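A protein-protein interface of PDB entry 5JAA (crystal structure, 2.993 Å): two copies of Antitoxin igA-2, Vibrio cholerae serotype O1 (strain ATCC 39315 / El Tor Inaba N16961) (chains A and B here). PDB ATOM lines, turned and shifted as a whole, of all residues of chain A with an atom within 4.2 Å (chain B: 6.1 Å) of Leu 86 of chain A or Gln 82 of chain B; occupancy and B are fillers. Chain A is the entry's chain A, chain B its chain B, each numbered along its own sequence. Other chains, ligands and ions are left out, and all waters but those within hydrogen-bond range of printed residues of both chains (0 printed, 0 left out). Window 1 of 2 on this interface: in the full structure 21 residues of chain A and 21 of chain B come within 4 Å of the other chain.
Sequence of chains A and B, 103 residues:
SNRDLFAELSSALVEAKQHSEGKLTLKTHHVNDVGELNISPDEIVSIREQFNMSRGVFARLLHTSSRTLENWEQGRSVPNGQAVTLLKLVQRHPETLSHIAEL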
ATOM      1  N   LEU A  62      24.338  27.577  12.057  1.00  0.00           N
ATOM      2  CA  LEU A  62      25.130  26.702  12.912  1.00  0.00           C
ATOM      3  C   LEU A  62      26.262  26.051  12.127  1.00  0.00           C
ATOM      4  O   LEU A  62      26.966  25.181  12.640  1.00  0.00           O
ATOM      5  CB  LEU A  62      24.247  25.635  13.552  1.00  0.00           C
ATOM      6  CG  LEU A  62      23.133  26.178  14.446  1.00  0.00           C
ATOM      7  CD1 LEU A  62      22.385  25.049  15.105  1.00  0.00           C
ATOM      8  CD2 LEU A  62      23.682  27.158  15.466  1.00  0.00           C
ATOM      9  N   HIS A  63      26.409  26.471  10.872  1.00  0.00           N
ATOM     10  CA  HIS A  63      27.447  25.971   9.972  1.00  0.00           C
ATOM     11  C   HIS A  63      27.437  24.449   9.890  1.00  0.00           C
ATOM     12  O   HIS A  63      28.464  23.794  10.072  1.00  0.00           O
ATOM     13  CB  HIS A  63      28.826  26.483  10.399  1.00  0.00           C
ATOM     14  CG  HIS A  63      29.027  27.949  10.150  1.00  0.00           C
ATOM     15  ND1 HIS A  63      28.649  28.918  11.055  1.00  0.00           N
ATOM     16  CD2 HIS A  63      29.558  28.610   9.093  1.00  0.00           C
ATOM     17  CE1 HIS A  63      28.942  30.111  10.569  1.00  0.00           C
ATOM     18  NE2 HIS A  63      29.494  29.952   9.380  1.00  0.00           N
ATOM     19  N   THR A  64      26.251  23.907   9.623  1.00  0.00           N
ATOM     20  CA  THR A  64      26.052  22.481   9.386  1.00  0.00           C
ATOM     21  C   THR A  64      24.962  22.296   8.327  1.00  0.00           C
ATOM     22  O   THR A  64      24.237  23.237   8.008  1.00  0.00           O
ATOM     23  CB  THR A  64      25.659  21.731  10.671  1.00  0.00           C
ATOM     24  OG1 THR A  64      25.628  20.320  10.416  1.00  0.00           O
ATOM     25  CG2 THR A  64      24.290  22.189  11.157  1.00  0.00           C
ATOM     26  N   ASN A  80      27.389  17.147  18.408  1.00  0.00           N
ATOM     27  CA  ASN A  80      28.605  17.124  19.198  1.00  0.00           C
ATOM     28  C   ASN A  80      28.592  18.173  20.306  1.00  0.00           C
ATOM     29  O   ASN A  80      27.626  18.919  20.462  1.00  0.00           O
ATOM     30  CB  ASN A  80      29.821  17.327  18.296  1.00  0.00           C
ATOM     31  CG  ASN A  80      29.779  18.641  17.558  1.00  0.00           C
ATOM     32  OD1 ASN A  80      30.157  19.683  18.097  1.00  0.00           O
ATOM     33  ND2 ASN A  80      29.307  18.606  16.317  1.00  0.00           N
ATOM     34  N   GLN A  82      30.427  21.021  20.981  1.00  0.00           N
ATOM     35  CA  GLN A  82      30.389  22.425  20.592  1.00  0.00           C
ATOM     36  C   GLN A  82      29.023  22.790  20.010  1.00  0.00           C
ATOM     37  O   GLN A  82      28.508  23.888  20.244  1.00  0.00           O
ATOM     38  CB  GLN A  82      31.495  22.737  19.588  1.00  0.00           C
ATOM     39  CG  GLN A  82      32.893  22.577  20.144  1.00  0.00           C
ATOM     40  CD  GLN A  82      33.311  21.127  20.268  1.00  0.00           C
ATOM     41  OE1 GLN A  82      33.082  20.324  19.365  1.00  0.00           O
ATOM     42  NE2 GLN A  82      33.920  20.782  21.397  1.00  0.00           N
ATOM     43  N   ALA A  83      28.440  21.860  19.259  1.00  0.00           N
ATOM     44  CA  ALA A  83      27.098  22.046  18.724  1.00  0.00           C
ATOM     45  C   ALA A  83      26.101  22.306  19.847  1.00  0.00           C
ATOM     46  O   ALA A  83      25.389  23.318  19.842  1.00  0.00           O
ATOM     47  CB  ALA A  83      26.678  20.834  17.909  1.00  0.00           C
ATOM     48  N   VAL A  84      26.060  21.393  20.813  1.00  0.00           N
ATOM     49  CA  VAL A  84      25.156  21.532  21.946  1.00  0.00           C
ATOM     50  C   VAL A  84      25.430  22.838  22.681  1.00  0.00           C
ATOM     51  O   VAL A  84      24.506  23.519  23.115  1.00  0.00           O
ATOM     52  CB  VAL A  84      25.276  20.347  22.927  1.00  0.00           C
ATOM     53  CG1 VAL A  84      24.318  20.528  24.098  1.00  0.00           C
ATOM     54  CG2 VAL A  84      24.992  19.033  22.210  1.00  0.00           C
ATOM     55  N   THR A  85      26.704  23.192  22.801  1.00  0.00           N
ATOM     56  CA  THR A  85      27.074  24.441  23.447  1.00  0.00           C
ATOM     57  C   THR A  85      26.449  25.646  22.746  1.00  0.00           C
ATOM     58  O   THR A  85      25.830  26.477  23.395  1.00  0.00           O
ATOM     59  CB  THR A  85      28.597  24.611  23.497  1.00  0.00           C
ATOM     60  OG1 THR A  85      29.156  23.613  24.361  1.00  0.00           O
ATOM     61  CG2 THR A  85      28.959  25.990  24.022  1.00  0.00           C
ATOM     62  N   LEU A  86      26.602  25.731  21.427  1.00  0.00           N
ATOM     63  CA  LEU A  86      25.992  26.818  20.659  1.00  0.00           C
ATOM     64  C   LEU A  86      24.472  26.836  20.801  1.00  0.00           C
ATOM     65  O   LEU A  86      23.870  27.894  20.969  1.00  0.00           O
ATOM     66  CB  LEU A  86      26.360  26.706  19.180  1.00  0.00           C
ATOM     67  CG  LEU A  86      27.782  27.078  18.767  1.00  0.00           C
ATOM     68  CD1 LEU A  86      27.948  26.939  17.261  1.00  0.00           C
ATOM     69  CD2 LEU A  86      28.121  28.485  19.218  1.00  0.00           C
ATOM     70  N   LEU A  87      23.858  25.660  20.728  1.00  0.00           N
ATOM     71  CA  LEU A  87      22.409  25.551  20.826  1.00  0.00           C
ATOM     72  C   LEU A  87      21.893  26.062  22.166  1.00  0.00           C
ATOM     73  O   LEU A  87      20.939  26.841  22.222  1.00  0.00           O
ATOM     74  CB  LEU A  87      21.978  24.104  20.613  1.00  0.00           C
ATOM     75  CG  LEU A  87      22.078  23.599  19.175  1.00  0.00           C
ATOM     76  CD1 LEU A  87      21.919  22.091  19.117  1.00  0.00           C
ATOM     77  CD2 LEU A  87      21.016  24.273  18.331  1.00  0.00           C
ATOM     78  N   LYS A  88      22.532  25.617  23.245  1.00  0.00           N
ATOM     79  CA  LYS A  88      22.171  26.054  24.590  1.00  0.00           C
ATOM     80  C   LYS A  88      22.399  27.553  24.723  1.00  0.00           C
ATOM     81  O   LYS A  88      21.596  28.275  25.326  1.00  0.00           O
ATOM     82  CB  LYS A  88      22.983  25.292  25.641  1.00  0.00           C
ATOM     83  CG  LYS A  88      22.466  23.894  25.960  1.00  0.00           C
ATOM     84  CD  LYS A  88      21.162  23.967  26.738  1.00  0.00           C
ATOM     85  CE  LYS A  88      20.689  22.592  27.175  1.00  0.00           C
ATOM     86  NZ  LYS A  88      19.391  22.668  27.902  1.00  0.00           N
ATOM     87  N   LEU A  89      23.494  28.008  24.124  1.00  0.00           N
ATOM     88  CA  LEU A  89      23.872  29.415  24.123  1.00  0.00           C
ATOM     89  C   LEU A  89      22.802  30.302  23.495  1.00  0.00           C
ATOM     90  O   LEU A  89      22.437  31.327  24.069  1.00  0.00           O
ATOM     91  CB  LEU A  89      25.197  29.600  23.386  1.00  0.00           C
ATOM     92  CG  LEU A  89      26.041  30.788  23.826  1.00  0.00           C
ATOM     93  CD1 LEU A  89      26.362  30.656  25.303  1.00  0.00           C
ATOM     94  CD2 LEU A  89      27.315  30.857  23.001  1.00  0.00           C
ATOM     95  N   VAL A  90      22.300  29.913  22.322  1.00  0.00           N
ATOM     96  CA  VAL A  90      21.269  30.704  21.651  1.00  0.00           C
ATOM     97  C   VAL A  90      19.911  30.496  22.316  1.00  0.00           C
ATOM     98  O   VAL A  90      19.016  31.334  22.191  1.00  0.00           O
ATOM     99  CB  VAL A  90      21.157  30.376  20.135  1.00  0.00           C
ATOM    100  CG1 VAL A  90      22.461  30.688  19.418  1.00  0.00           C
ATOM    101  CG2 VAL A  90      20.760  28.929  19.909  1.00  0.00           C
ATOM    102  N   ILE A 100      26.689  35.361  15.713  1.00  0.00           N
ATOM    103  CA  ILE A 100      27.060  34.271  14.820  1.00  0.00           C
ATOM    104  C   ILE A 100      26.819  34.639  13.358  1.00  0.00           C
ATOM    105  O   ILE A 100      27.660  34.376  12.498  1.00  0.00           O
ATOM    106  CB  ILE A 100      26.275  32.985  15.156  1.00  0.00           C
ATOM    107  CG1 ILE A 100      26.688  32.456  16.532  1.00  0.00           C
ATOM    108  CG2 ILE A 100      26.498  31.930  14.096  1.00  0.00           C
ATOM    109  CD1 ILE A 100      26.055  31.130  16.897  1.00  0.00           C
ATOM    110  N   ASN B  80      35.833  21.009  14.225  1.00  0.00           N
ATOM    111  CA  ASN B  80      34.623  20.935  13.420  1.00  0.00           C
ATOM    112  C   ASN B  80      33.968  22.301  13.263  1.00  0.00           C
ATOM    113  O   ASN B  80      34.464  23.302  13.777  1.00  0.00           O
ATOM    114  CB  ASN B  80      33.627  19.952  14.035  1.00  0.00           C
ATOM    115  CG  ASN B  80      33.263  20.309  15.460  1.00  0.00           C
ATOM    116  OD1 ASN B  80      32.432  21.184  15.701  1.00  0.00           O
ATOM    117  ND2 ASN B  80      33.887  19.631  16.416  1.00  0.00           N
ATOM    118  N   GLY B  81      32.843  22.329  12.556  1.00  0.00           N
ATOM    119  CA  GLY B  81      32.168  23.574  12.241  1.00  0.00           C
ATOM    120  C   GLY B  81      31.728  24.358  13.459  1.00  0.00           C
ATOM    121  O   GLY B  81      32.047  25.543  13.603  1.00  0.00           O
ATOM    122  N   GLN B  82      30.996  23.696  14.346  1.00  0.00           N
ATOM    123  CA  GLN B  82      30.470  24.355  15.530  1.00  0.00           C
ATOM    124  C   GLN B  82      31.611  24.769  16.446  1.00  0.00           C
ATOM    125  O   GLN B  82      31.509  25.757  17.173  1.00  0.00           O
ATOM    126  CB  GLN B  82      29.486  23.443  16.263  1.00  0.00           C
ATOM    127  CG  GLN B  82      28.232  23.112  15.463  1.00  0.00           C
ATOM    128  CD  GLN B  82      28.475  22.069  14.394  1.00  0.00           C
ATOM    129  OE1 GLN B  82      29.217  21.110  14.604  1.00  0.00           O
ATOM    130  NE2 GLN B  82      27.857  22.255  13.234  1.00  0.00           N
ATOM    131  N   ALA B  83      32.702  24.013  16.393  1.00  0.00           N
ATOM    132  CA  ALA B  83      33.895  24.344  17.154  1.00  0.00           C
ATOM    133  C   ALA B  83      34.487  25.675  16.689  1.00  0.00           C
ATOM    134  O   ALA B  83      34.725  26.573  17.501  1.00  0.00           O
ATOM    135  CB  ALA B  83      34.914  23.231  17.034  1.00  0.00           C
ATOM    136  N   VAL B  84      34.721  25.798  15.386  1.00  0.00           N
ATOM    137  CA  VAL B  84      35.268  27.034  14.834  1.00  0.00           C
ATOM    138  C   VAL B  84      34.321  28.199  15.083  1.00  0.00           C
ATOM    139  O   VAL B  84      34.758  29.301  15.415  1.00  0.00           O
ATOM    140  CB  VAL B  84      35.542  26.918  13.326  1.00  0.00           C
ATOM    141  CG1 VAL B  84      36.243  28.166  12.819  1.00  0.00           C
ATOM    142  CG2 VAL B  84      36.385  25.688  13.038  1.00  0.00           C
ATOM    143  N   THR B  85      33.027  27.945  14.930  1.00  0.00           N
ATOM    144  CA  THR B  85      32.011  28.956  15.196  1.00  0.00           C
ATOM    145  C   THR B  85      32.127  29.482  16.616  1.00  0.00           C
ATOM    146  O   THR B  85      32.182  30.689  16.852  1.00  0.00           O
ATOM    147  CB  THR B  85      30.595  28.397  15.004  1.00  0.00           C
ATOM    148  OG1 THR B  85      30.506  27.724  13.742  1.00  0.00           O
ATOM    149  CG2 THR B  85      29.568  29.512  15.073  1.00  0.00           C
ATOM    150  N   LEU B  86      32.170  28.548  17.556  1.00  0.00           N
ATOM    151  CA  LEU B  86      32.246  28.866  18.970  1.00  0.00           C
ATOM    152  C   LEU B  86      33.517  29.645  19.282  1.00  0.00           C
ATOM    153  O   LEU B  86      33.491  30.639  20.011  1.00  0.00           O
ATOM    154  CB  LEU B  86      32.183  27.578  19.781  1.00  0.00           C
ATOM    155  CG  LEU B  86      32.045  27.692  21.290  1.00  0.00           C
ATOM    156  CD1 LEU B  86      30.862  28.567  21.633  1.00  0.00           C
ATOM    157  CD2 LEU B  86      31.889  26.302  21.881  1.00  0.00           C
ATOM    158  N   LEU B  87      34.626  29.199  18.704  1.00  0.00           N
ATOM    159  CA  LEU B  87      35.909  29.846  18.908  1.00  0.00           C
ATOM    160  C   LEU B  87      35.888  31.286  18.422  1.00  0.00           C
ATOM    161  O   LEU B  87      36.280  32.192  19.155  1.00  0.00           O
ATOM    162  CB  LEU B  87      37.018  29.061  18.208  1.00  0.00           C
ATOM    163  CG  LEU B  87      37.509  27.825  18.965  1.00  0.00           C
ATOM    164  CD1 LEU B  87      38.474  27.016  18.116  1.00  0.00           C
ATOM    165  CD2 LEU B  87      38.166  28.231  20.276  1.00  0.00           C
ATOM    166  N   LEU B  89      33.302  33.123  17.963  1.00  0.00           N
ATOM    167  CA  LEU B  89      32.358  33.821  18.820  1.00  0.00           C
ATOM    168  C   LEU B  89      33.033  34.330  20.087  1.00  0.00           C
ATOM    169  O   LEU B  89      32.885  35.495  20.452  1.00  0.00           O
ATOM    170  CB  LEU B  89      31.192  32.904  19.180  1.00  0.00           C
ATOM    171  CG  LEU B  89      29.935  33.623  19.657  1.00  0.00           C
ATOM    172  CD1 LEU B  89      29.384  34.484  18.534  1.00  0.00           C
ATOM    173  CD2 LEU B  89      28.902  32.621  20.132  1.00  0.00           C
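Asn 80 of chain A touches Gln 82 of chain B, and with the chains exchanged Gln 82 of chain A touches Asn 80 of chain B. Gln 82 of chain B touches its own counterpart, Gln 82 of chain A. Thr 85 of chain A touches Leu 86 of chain B, and with the chains exchanged Leu 86 of chain A touches Thr 85 of chain B. Leu 89 of chain B touches its own counterpart, Leu 89 of chain A. Positions printed for both chains: 80, 82, 83, 84, 85, 86, 87 and 89. Of the 16 pairs that touch across the chains among the printed residues, 10 have their exchanged pair printed and touching as well.
Among the printed residues, pairs that only touch across the chains: His 63 of chain A with Gln 82 of chain B (3.6 Å), Thr 64 of chain A with Gln 82 of chain B (3.4 Å), Asn 80 of chain A with Asn 80 of chain B (3.6 Å), Gln 82 of chain A with Gln 82 of chain B (3.7 Å), Gln 82 of chain A with Ala 83 of chain B (3.6 Å), Ala 83 of chain A with Gln 82 of chain B (3.5 Å), Thr 85 of chain A with Leu 86 of chain B (3.6 Å), Leu 86 of chain A with Gln 82 of chain B (3.8 Å), Leu 86 of chain A with Thr 85 of chain B (3.7 Å), Leu 86 of chain A with Leu 86 of chain B (3.7 Å), Leu 89 of chain A with Leu 89 of chain B (3.7 Å) and Ile 100 of chain A with Leu 89 of chain B (3.9 Å).
O of Leu 62 of chain A lies within hydrogen-bond range of NE2 of Gln 82 of chain B (3.1 Å). The side-chain hydroxyl of Thr 85 of chain B is in hydrogen-bond range of a ring nitrogen (ND1) of His 63 of chain A (3.5 Å). OE1 of Gln 82 of chain B lies within hydrogen-bond range of ND2 of Asn 80 of chain A (3.0 Å). ND2 of Asn 80 of chain B is in hydrogen-bond range of OE1 of Gln 82 of chain A, 3.1 Å away.
The backbone NH (N) of Gln 82 of chain A lies within hydrogen-bond range of the side-chain amide oxygen (OD1) of Asn 80 of chain A (3.2 Å). OD1 of Asn 80 of chain A sits at hydrogen-bond distance from N of Ala 83 of chain A (3.0 Å). The side-chain amide oxygen (OD1) of Asn 80 of chain B is in hydrogen-bond range of the backbone NH (N) of Gln 82 of chain B (3.2 Å). The side-chain amide oxygen (OD1) of Asn 80 of chain B is in hydrogen-bond range of the backbone NH (N) of Ala 83 of chain B, at 2.9 Å. OG1 of Thr 85 of chain B sits at hydrogen-bond distance from O of Gly 81 of chain B, at 2.7 Å.
Of the 9 printed residues of chain B, 6 touch a printed residue of chain A. Hydrophobic or aromatic side chains of chain B within 4 Å of the printed part of chain A: Ala 83, Leu 86 and Leu 89. Printed residues of chain A that touch a printed residue of chain B: Leu 62, His 63, Thr 64, Asn 80, Gln 82, Ala 83, Thr 85, Leu 86, Leu 89 and Ile 100. Hydrophobic or aromatic side chains of chain A that line the printed part of chain B: His 63, Ala 83, Leu 86, Leu 89 and Ile 100. Among the printed residues, 16 pairs touch across the chains.
Leu 86 of chain A touches just these residues of chain B: Gln 82 (3.8 Å), Thr 85 (3.7 Å) and Leu 86 (3.7 Å). Gln 82 of chain B touches just these residues of chain A: Leu 62 (3.1 Å), His 63 (3.6 Å), Thr 64 (3.4 Å), Asn 80 (3.0 Å), Gln 82 (3.7 Å), Ala 83 (3.5 Å) and Leu 86 (3.8 Å). Of the printed residues of chain A, Ala 83 of chain B touches Gln 82. Printed residues of chain B within 4 Å of Gln 82 of chain A: Asn 80, Gln 82 and Ala 83. Of the printed residues of chain A, Asn 80 of chain B touches Asn 80 (3.6 Å) and Gln 82 (3.1 Å). Val 84 of chain B touches none of the printed residues of chain A. The nearest residue of chain B that does not touch Leu 86 of chain A is Leu 89 of chain B (4.3 Å). The nearest printed residue of chain A that does not touch Gln 82 of chain B is Val 84 of chain A (6.0 Å). The nearest printed residue of chain B that does not touch Gln 82 of chain A is Leu 86 of chain B (4.2 Å).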
